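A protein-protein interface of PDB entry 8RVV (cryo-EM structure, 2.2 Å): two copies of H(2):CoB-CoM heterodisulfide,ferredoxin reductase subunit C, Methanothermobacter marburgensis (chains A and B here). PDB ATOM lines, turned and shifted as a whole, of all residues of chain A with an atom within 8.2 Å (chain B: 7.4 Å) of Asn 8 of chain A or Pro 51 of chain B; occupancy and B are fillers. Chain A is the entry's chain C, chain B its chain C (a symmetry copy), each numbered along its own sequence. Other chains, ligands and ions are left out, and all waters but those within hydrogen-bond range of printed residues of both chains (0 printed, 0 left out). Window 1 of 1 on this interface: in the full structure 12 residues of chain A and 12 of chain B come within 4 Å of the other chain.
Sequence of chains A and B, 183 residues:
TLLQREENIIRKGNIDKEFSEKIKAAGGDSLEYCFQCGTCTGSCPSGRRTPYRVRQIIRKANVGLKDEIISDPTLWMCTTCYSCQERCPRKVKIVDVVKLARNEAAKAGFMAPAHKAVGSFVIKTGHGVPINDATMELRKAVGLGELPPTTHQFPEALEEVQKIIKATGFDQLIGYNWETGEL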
ATOM      1  N   THR A   1      28.412  28.487  14.833  1.00  0.00           N
ATOM      2  CA  THR A   1      27.008  28.103  14.809  1.00  0.00           C
ATOM      3  C   THR A   1      26.254  28.720  15.981  1.00  0.00           C
ATOM      4  O   THR A   1      26.799  28.870  17.072  1.00  0.00           O
ATOM      5  CB  THR A   1      26.839  26.574  14.859  1.00  0.00           C
ATOM      6  OG1 THR A   1      25.453  26.236  14.740  1.00  0.00           O
ATOM      7  CG2 THR A   1      27.379  26.010  16.165  1.00  0.00           C
ATOM      8  N   LEU A   2      24.995  29.078  15.743  1.00  0.00           N
ATOM      9  CA  LEU A   2      24.119  29.567  16.794  1.00  0.00           C
ATOM     10  C   LEU A   2      23.428  28.444  17.552  1.00  0.00           C
ATOM     11  O   LEU A   2      22.674  28.720  18.488  1.00  0.00           O
ATOM     12  CB  LEU A   2      23.063  30.506  16.206  1.00  0.00           C
ATOM     13  CG  LEU A   2      23.579  31.867  15.745  1.00  0.00           C
ATOM     14  CD1 LEU A   2      22.543  32.563  14.884  1.00  0.00           C
ATOM     15  CD2 LEU A   2      23.954  32.726  16.937  1.00  0.00           C
ATOM     16  N   LEU A   3      23.665  27.193  17.173  1.00  0.00           N
ATOM     17  CA  LEU A   3      23.007  26.075  17.831  1.00  0.00           C
ATOM     18  C   LEU A   3      23.508  25.943  19.262  1.00  0.00           C
ATOM     19  O   LEU A   3      24.708  26.029  19.529  1.00  0.00           O
ATOM     20  CB  LEU A   3      23.326  24.773  17.099  1.00  0.00           C
ATOM     21  CG  LEU A   3      22.786  23.487  17.726  1.00  0.00           C
ATOM     22  CD1 LEU A   3      21.268  23.469  17.704  1.00  0.00           C
ATOM     23  CD2 LEU A   3      23.344  22.278  17.009  1.00  0.00           C
ATOM     24  N   GLN A   4      22.571  25.733  20.186  1.00  0.00           N
ATOM     25  CA  GLN A   4      22.889  25.382  21.562  1.00  0.00           C
ATOM     26  C   GLN A   4      21.583  24.847  22.136  1.00  0.00           C
ATOM     27  O   GLN A   4      20.621  25.603  22.294  1.00  0.00           O
ATOM     28  CB  GLN A   4      23.436  26.559  22.358  1.00  0.00           C
ATOM     29  CG  GLN A   4      23.892  26.177  23.753  1.00  0.00           C
ATOM     30  CD  GLN A   4      25.058  25.211  23.737  1.00  0.00           C
ATOM     31  OE1 GLN A   4      26.123  25.514  23.207  1.00  0.00           O
ATOM     32  NE2 GLN A   4      24.865  24.043  24.332  1.00  0.00           N
ATOM     33  N   ARG A   5      21.552  23.550  22.431  1.00  0.00           N
ATOM     34  CA  ARG A   5      20.314  22.845  22.731  1.00  0.00           C
ATOM     35  C   ARG A   5      19.916  22.983  24.195  1.00  0.00           C
ATOM     36  O   ARG A   5      18.803  22.586  24.550  1.00  0.00           O
ATOM     37  CB  ARG A   5      20.564  21.365  22.421  1.00  0.00           C
ATOM     38  CG  ARG A   5      21.177  21.095  21.048  1.00  0.00           C
ATOM     39  CD  ARG A   5      21.988  19.807  21.025  1.00  0.00           C
ATOM     40  NE  ARG A   5      21.335  18.763  20.241  1.00  0.00           N
ATOM     41  CZ  ARG A   5      21.114  17.521  20.656  1.00  0.00           C
ATOM     42  NH1 ARG A   5      21.486  17.109  21.856  1.00  0.00           N
ATOM     43  NH2 ARG A   5      20.501  16.667  19.841  1.00  0.00           N
ATOM     44  N   GLU A   6      20.783  23.524  25.049  1.00  0.00           N
ATOM     45  CA  GLU A   6      20.487  23.660  26.468  1.00  0.00           C
ATOM     46  C   GLU A   6      20.111  25.072  26.898  1.00  0.00           C
ATOM     47  O   GLU A   6      19.247  25.235  27.762  1.00  0.00           O
ATOM     48  CB  GLU A   6      21.684  23.170  27.294  1.00  0.00           C
ATOM     49  CG  GLU A   6      22.020  21.692  27.147  1.00  0.00           C
ATOM     50  CD  GLU A   6      20.865  20.785  27.517  1.00  0.00           C
ATOM     51  OE1 GLU A   6      20.162  21.085  28.505  1.00  0.00           O
ATOM     52  OE2 GLU A   6      20.664  19.766  26.823  1.00  0.00           O
ATOM     53  N   GLU A   7      20.729  26.091  26.308  1.00  0.00           N
ATOM     54  CA  GLU A   7      20.557  27.460  26.775  1.00  0.00           C
ATOM     55  C   GLU A   7      19.269  28.156  26.364  1.00  0.00           C
ATOM     56  O   GLU A   7      18.978  29.234  26.891  1.00  0.00           O
ATOM     57  CB  GLU A   7      21.743  28.278  26.259  1.00  0.00           C
ATOM     58  CG  GLU A   7      22.848  28.467  27.274  1.00  0.00           C
ATOM     59  CD  GLU A   7      24.193  28.704  26.624  1.00  0.00           C
ATOM     60  OE1 GLU A   7      25.218  28.295  27.210  1.00  0.00           O
ATOM     61  OE2 GLU A   7      24.228  29.302  25.527  1.00  0.00           O
ATOM     62  N   ASN A   8      18.492  27.579  25.449  1.00  0.00           N
ATOM     63  CA  ASN A   8      17.372  28.279  24.834  1.00  0.00           C
ATOM     64  C   ASN A   8      16.031  27.633  25.146  1.00  0.00           C
ATOM     65  O   ASN A   8      15.041  27.907  24.464  1.00  0.00           O
ATOM     66  CB  ASN A   8      17.588  28.365  23.325  1.00  0.00           C
ATOM     67  CG  ASN A   8      18.808  29.180  22.965  1.00  0.00           C
ATOM     68  OD1 ASN A   8      18.821  30.395  23.127  1.00  0.00           O
ATOM     69  ND2 ASN A   8      19.848  28.513  22.487  1.00  0.00           N
ATOM     70  N   ILE A   9      15.973  26.788  26.171  1.00  0.00           N
ATOM     71  CA  ILE A   9      14.726  26.167  26.590  1.00  0.00           C
ATOM     72  C   ILE A   9      14.818  25.885  28.080  1.00  0.00           C
ATOM     73  O   ILE A   9      15.897  25.617  28.611  1.00  0.00           O
ATOM     74  CB  ILE A   9      14.435  24.878  25.785  1.00  0.00           C
ATOM     75  CG1 ILE A   9      12.980  24.450  25.966  1.00  0.00           C
ATOM     76  CG2 ILE A   9      15.372  23.762  26.206  1.00  0.00           C
ATOM     77  CD1 ILE A   9      12.493  23.520  24.897  1.00  0.00           C
ATOM     78  N   ILE A  10      13.676  25.951  28.756  1.00  0.00           N
ATOM     79  CA  ILE A  10      13.591  25.697  30.188  1.00  0.00           C
ATOM     80  C   ILE A  10      12.747  24.451  30.390  1.00  0.00           C
ATOM     81  O   ILE A  10      11.597  24.393  29.940  1.00  0.00           O
ATOM     82  CB  ILE A  10      12.998  26.889  30.956  1.00  0.00           C
ATOM     83  CG1 ILE A  10      13.717  28.184  30.577  1.00  0.00           C
ATOM     84  CG2 ILE A  10      13.108  26.655  32.452  1.00  0.00           C
ATOM     85  CD1 ILE A  10      13.095  29.419  31.176  1.00  0.00           C
ATOM     86  N   ARG A  11      13.318  23.458  31.062  1.00  0.00           N
ATOM     87  CA  ARG A  11      12.618  22.249  31.462  1.00  0.00           C
ATOM     88  C   ARG A  11      12.786  22.073  32.965  1.00  0.00           C
ATOM     89  O   ARG A  11      13.416  22.891  33.639  1.00  0.00           O
ATOM     90  CB  ARG A  11      13.141  21.027  30.698  1.00  0.00           C
ATOM     91  CG  ARG A  11      12.954  21.116  29.200  1.00  0.00           C
ATOM     92  CD  ARG A  11      12.827  19.743  28.575  1.00  0.00           C
ATOM     93  NE  ARG A  11      12.701  19.812  27.125  1.00  0.00           N
ATOM     94  CZ  ARG A  11      13.709  20.032  26.293  1.00  0.00           C
ATOM     95  NH1 ARG A  11      14.945  20.203  26.732  1.00  0.00           N
ATOM     96  NH2 ARG A  11      13.472  20.087  24.987  1.00  0.00           N
ATOM     97  N   ASN A  14      16.210  22.306  34.758  1.00  0.00           N
ATOM     98  CA  ASN A  14      16.793  23.601  35.078  1.00  0.00           C
ATOM     99  C   ASN A  14      16.248  24.195  36.368  1.00  0.00           C
ATOM    100  O   ASN A  14      16.661  25.293  36.748  1.00  0.00           O
ATOM    101  CB  ASN A  14      16.545  24.586  33.933  1.00  0.00           C
ATOM    102  CG  ASN A  14      16.937  24.026  32.583  1.00  0.00           C
ATOM    103  OD1 ASN A  14      16.085  23.616  31.798  1.00  0.00           O
ATOM    104  ND2 ASN A  14      18.232  24.015  32.302  1.00  0.00           N
ATOM    105  N   SER B  46      12.964  26.779  15.657  1.00  0.00           N
ATOM    106  CA  SER B  46      14.314  27.316  15.741  1.00  0.00           C
ATOM    107  C   SER B  46      14.534  28.090  17.032  1.00  0.00           C
ATOM    108  O   SER B  46      15.669  28.178  17.508  1.00  0.00           O
ATOM    109  CB  SER B  46      14.613  28.204  14.532  1.00  0.00           C
ATOM    110  OG  SER B  46      13.792  29.352  14.511  1.00  0.00           O
ATOM    111  N   GLY B  47      13.472  28.647  17.614  1.00  0.00           N
ATOM    112  CA  GLY B  47      13.596  29.326  18.888  1.00  0.00           C
ATOM    113  C   GLY B  47      13.931  28.406  20.041  1.00  0.00           C
ATOM    114  O   GLY B  47      14.371  28.881  21.091  1.00  0.00           O
ATOM    115  N   ARG B  48      13.731  27.100  19.871  1.00  0.00           N
ATOM    116  CA  ARG B  48      14.052  26.140  20.916  1.00  0.00           C
ATOM    117  C   ARG B  48      15.530  25.782  20.960  1.00  0.00           C
ATOM    118  O   ARG B  48      15.986  25.230  21.964  1.00  0.00           O
ATOM    119  CB  ARG B  48      13.242  24.858  20.720  1.00  0.00           C
ATOM    120  CG  ARG B  48      11.746  25.054  20.736  1.00  0.00           C
ATOM    121  CD  ARG B  48      11.027  23.802  21.201  1.00  0.00           C
ATOM    122  NE  ARG B  48      11.070  22.731  20.211  1.00  0.00           N
ATOM    123  CZ  ARG B  48      10.281  22.653  19.149  1.00  0.00           C
ATOM    124  NH1 ARG B  48       9.383  23.587  18.883  1.00  0.00           N
ATOM    125  NH2 ARG B  48      10.393  21.609  18.334  1.00  0.00           N
ATOM    126  N   ARG B  49      16.284  26.076  19.901  1.00  0.00           N
ATOM    127  CA  ARG B  49      17.678  25.676  19.815  1.00  0.00           C
ATOM    128  C   ARG B  49      18.607  26.807  19.399  1.00  0.00           C
ATOM    129  O   ARG B  49      19.805  26.567  19.227  1.00  0.00           O
ATOM    130  CB  ARG B  49      17.835  24.504  18.833  1.00  0.00           C
ATOM    131  CG  ARG B  49      17.477  24.834  17.395  1.00  0.00           C
ATOM    132  CD  ARG B  49      16.967  23.612  16.661  1.00  0.00           C
ATOM    133  NE  ARG B  49      15.552  23.382  16.923  1.00  0.00           N
ATOM    134  CZ  ARG B  49      14.983  22.191  17.042  1.00  0.00           C
ATOM    135  NH1 ARG B  49      15.678  21.071  16.918  1.00  0.00           N
ATOM    136  NH2 ARG B  49      13.680  22.118  17.292  1.00  0.00           N
ATOM    137  N   THR B  50      18.098  28.014  19.223  1.00  0.00           N
ATOM    138  CA  THR B  50      18.921  29.163  18.876  1.00  0.00           C
ATOM    139  C   THR B  50      18.426  30.363  19.670  1.00  0.00           C
ATOM    140  O   THR B  50      17.359  30.293  20.292  1.00  0.00           O
ATOM    141  CB  THR B  50      18.873  29.457  17.373  1.00  0.00           C
ATOM    142  OG1 THR B  50      17.612  30.049  17.036  1.00  0.00           O
ATOM    143  CG2 THR B  50      19.064  28.189  16.561  1.00  0.00           C
ATOM    144  N   PRO B  51      19.158  31.468  19.686  1.00  0.00           N
ATOM    145  CA  PRO B  51      18.670  32.659  20.392  1.00  0.00           C
ATOM    146  C   PRO B  51      17.596  33.411  19.623  1.00  0.00           C
ATOM    147  O   PRO B  51      17.215  34.519  20.011  1.00  0.00           O
ATOM    148  CB  PRO B  51      19.935  33.514  20.560  1.00  0.00           C
ATOM    149  CG  PRO B  51      21.078  32.642  20.161  1.00  0.00           C
ATOM    150  CD  PRO B  51      20.538  31.643  19.213  1.00  0.00           C
ATOM    151  N   TYR B  52      17.105  32.829  18.533  1.00  0.00           N
ATOM    152  CA  TYR B  52      16.098  33.489  17.715  1.00  0.00           C
ATOM    153  C   TYR B  52      14.768  33.554  18.455  1.00  0.00           C
ATOM    154  O   TYR B  52      14.251  32.532  18.913  1.00  0.00           O
ATOM    155  CB  TYR B  52      15.942  32.742  16.392  1.00  0.00           C
ATOM    156  CG  TYR B  52      14.813  33.231  15.518  1.00  0.00           C
ATOM    157  CD1 TYR B  52      14.774  34.540  15.070  1.00  0.00           C
ATOM    158  CD2 TYR B  52      13.794  32.375  15.130  1.00  0.00           C
ATOM    159  CE1 TYR B  52      13.747  34.986  14.269  1.00  0.00           C
ATOM    160  CE2 TYR B  52      12.765  32.812  14.328  1.00  0.00           C
ATOM    161  CZ  TYR B  52      12.746  34.118  13.899  1.00  0.00           C
ATOM    162  OH  TYR B  52      11.719  34.560  13.100  1.00  0.00           O
ATOM    163  N   ARG B  53      14.220  34.761  18.573  1.00  0.00           N
ATOM    164  CA  ARG B  53      12.931  34.999  19.220  1.00  0.00           C
ATOM    165  C   ARG B  53      12.084  35.816  18.249  1.00  0.00           C
ATOM    166  O   ARG B  53      12.296  37.021  18.098  1.00  0.00           O
ATOM    167  CB  ARG B  53      13.095  35.726  20.551  1.00  0.00           C
ATOM    168  CG  ARG B  53      14.065  35.079  21.520  1.00  0.00           C
ATOM    169  CD  ARG B  53      13.452  33.882  22.218  1.00  0.00           C
ATOM    170  NE  ARG B  53      14.395  33.259  23.138  1.00  0.00           N
ATOM    171  CZ  ARG B  53      15.304  32.359  22.794  1.00  0.00           C
ATOM    172  NH1 ARG B  53      15.404  31.914  21.553  1.00  0.00           N
ATOM    173  NH2 ARG B  53      16.134  31.890  23.720  1.00  0.00           N
ATOM    174  N   VAL B  54      11.126  35.161  17.595  1.00  0.00           N
ATOM    175  CA  VAL B  54      10.346  35.831  16.560  1.00  0.00           C
ATOM    176  C   VAL B  54       9.471  36.928  17.157  1.00  0.00           C
ATOM    177  O   VAL B  54       9.268  37.979  16.537  1.00  0.00           O
ATOM    178  CB  VAL B  54       9.515  34.806  15.764  1.00  0.00           C
ATOM    179  CG1 VAL B  54       8.679  33.935  16.687  1.00  0.00           C
ATOM    180  CG2 VAL B  54       8.636  35.515  14.756  1.00  0.00           C
ATOM    181  N   GLN B  56      10.136  38.906  19.640  1.00  0.00           N
ATOM    182  CA  GLN B  56      10.962  40.093  19.815  1.00  0.00           C
ATOM    183  C   GLN B  56      11.304  40.736  18.480  1.00  0.00           C
ATOM    184  O   GLN B  56      11.456  41.957  18.410  1.00  0.00           O
ATOM    185  CB  GLN B  56      12.231  39.739  20.584  1.00  0.00           C
ATOM    186  CG  GLN B  56      11.975  39.342  22.024  1.00  0.00           C
ATOM    187  CD  GLN B  56      13.198  38.754  22.696  1.00  0.00           C
ATOM    188  OE1 GLN B  56      14.329  39.006  22.283  1.00  0.00           O
ATOM    189  NE2 GLN B  56      12.976  37.956  23.732  1.00  0.00           N
ATOM    190  N   ASP B  72      21.197  41.460  12.982  1.00  0.00           N
ATOM    191  CA  ASP B  72      21.058  40.322  13.881  1.00  0.00           C
ATOM    192  C   ASP B  72      21.256  39.015  13.120  1.00  0.00           C
ATOM    193  O   ASP B  72      20.525  38.757  12.160  1.00  0.00           O
ATOM    194  CB  ASP B  72      19.686  40.337  14.532  1.00  0.00           C
ATOM    195  CG  ASP B  72      19.568  39.342  15.662  1.00  0.00           C
ATOM    196  OD1 ASP B  72      20.597  38.747  16.042  1.00  0.00           O
ATOM    197  OD2 ASP B  72      18.445  39.154  16.172  1.00  0.00           O
ATOM    198  N   THR B  74      20.450  36.060  14.215  1.00  0.00           N
ATOM    199  CA  THR B  74      19.315  35.186  14.488  1.00  0.00           C
ATOM    200  C   THR B  74      18.170  35.418  13.515  1.00  0.00           C
ATOM    201  O   THR B  74      17.322  34.534  13.353  1.00  0.00           O
ATOM    202  CB  THR B  74      18.817  35.381  15.922  1.00  0.00           C
ATOM    203  OG1 THR B  74      18.441  36.747  16.123  1.00  0.00           O
ATOM    204  CG2 THR B  74      19.890  34.998  16.922  1.00  0.00           C
ATOM    205  N   MET B  77      17.604  32.515  11.258  1.00  0.00           N
ATOM    206  CA  MET B  77      17.275  31.209  11.810  1.00  0.00           C
ATOM    207  C   MET B  77      15.870  30.743  11.455  1.00  0.00           C
ATOM    208  O   MET B  77      15.549  29.575  11.689  1.00  0.00           O
ATOM    209  CB  MET B  77      17.420  31.227  13.335  1.00  0.00           C
ATOM    210  CG  MET B  77      18.846  31.409  13.814  1.00  0.00           C
ATOM    211  SD  MET B  77      19.930  30.071  13.298  1.00  0.00           S
ATOM    212  CE  MET B  77      20.730  30.818  11.886  1.00  0.00           C
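The backbone NH (N) of Gln 4 of chain A sits at hydrogen-bond distance from the backbone carbonyl oxygen (O) of Arg 49 of chain B (3.0 Å). The side-chain amide oxygen (OD1) of Asn 8 of chain A is in hydrogen-bond range of the guanidinium group (NH2) of Arg 53 of chain B. The side-chain amide oxygen (OD1) of Asn 8 of chain A sits close to the backbone carbonyl oxygen (O) of Thr 50 of chain B.
The backbone carbonyl oxygen (O) of Ser 46 of chain B is in hydrogen-bond range of the side-chain hydroxyl (OG1) of Thr 50 of chain B. The guanidinium group (NH1) of Arg 53 of chain B sits at hydrogen-bond distance from the backbone carbonyl oxygen (O) of Thr 50 of chain B (2.8 Å). OG1 of Thr 50 of chain B lies close to N of Tyr 52 of chain B (3.2 Å). The side-chain hydroxyl (OG) of Ser 46 of chain B lies close to the backbone carbonyl oxygen (O) of Met 77 of chain B, at 3.3 Å. The backbone NH (N) of Leu 3 of chain A sits at hydrogen-bond distance from the side-chain hydroxyl (OG1) of Thr 1 of chain A (3.2 Å). The backbone carbonyl oxygen of Gln 4 of chain A is in hydrogen-bond range of the side-chain amide nitrogen of Asn 8 of chain A, at 3.0 Å.
Among the printed residues, pairs that only touch across the chains: Leu 3 of chain A with Arg 49 of chain B, Asn 8 of chain A with Pro 51 of chain B, Asn 8 of chain A with Gly 47 of chain B, Leu 2 of chain A with Arg 49 of chain B, Leu 2 of chain A with Pro 51 of chain B, Asn 8 of chain A with Arg 49 of chain B, Asn 8 of chain A with Arg 48 of chain B, Leu 2 of chain A with Thr 50 of chain B, Leu 2 of chain A with Met 77 of chain B and Ile 9 of chain A with Arg 48 of chain B.
Of the printed residues of chain A, Arg 48 of chain B touches Asn 8 and Ile 9. Of the printed residues of chain B, Gln 4 of chain A touches Arg 49. Arg 11 of chain A touches none of the printed residues of chain B. Ile 10 of chain A touches none of the printed residues of chain B. The nearest residue of chain A that does not touch Pro 51 of chain B is Leu 3 of chain A (5.8 Å). The nearest printed residue of chain B that does not touch Gln 4 of chain A is Thr 50 of chain B (4.6 Å).
Printed residues of chain A that touch a printed residue of chain B: Leu 2, Leu 3, Gln 4, Asn 8 and Ile 9. Of the 13 printed residues of chain B, 7 touch a printed residue of chain A. Printed residues of chain B that touch a printed residue of chain A: Gly 47, Arg 48, Arg 49, Thr 50, Pro 51, Arg 53 and Met 77. Among the printed residues, 13 pairs touch across the chains. Among the printed residues, no Asp or Glu carboxylate lies within 4 Å of a Lys or Arg side-chain nitrogen of the other chain.
No position is printed for both chains. Of the 13 pairs that touch across the chains among the printed residues, none has its exchanged pair printed and touching as well.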
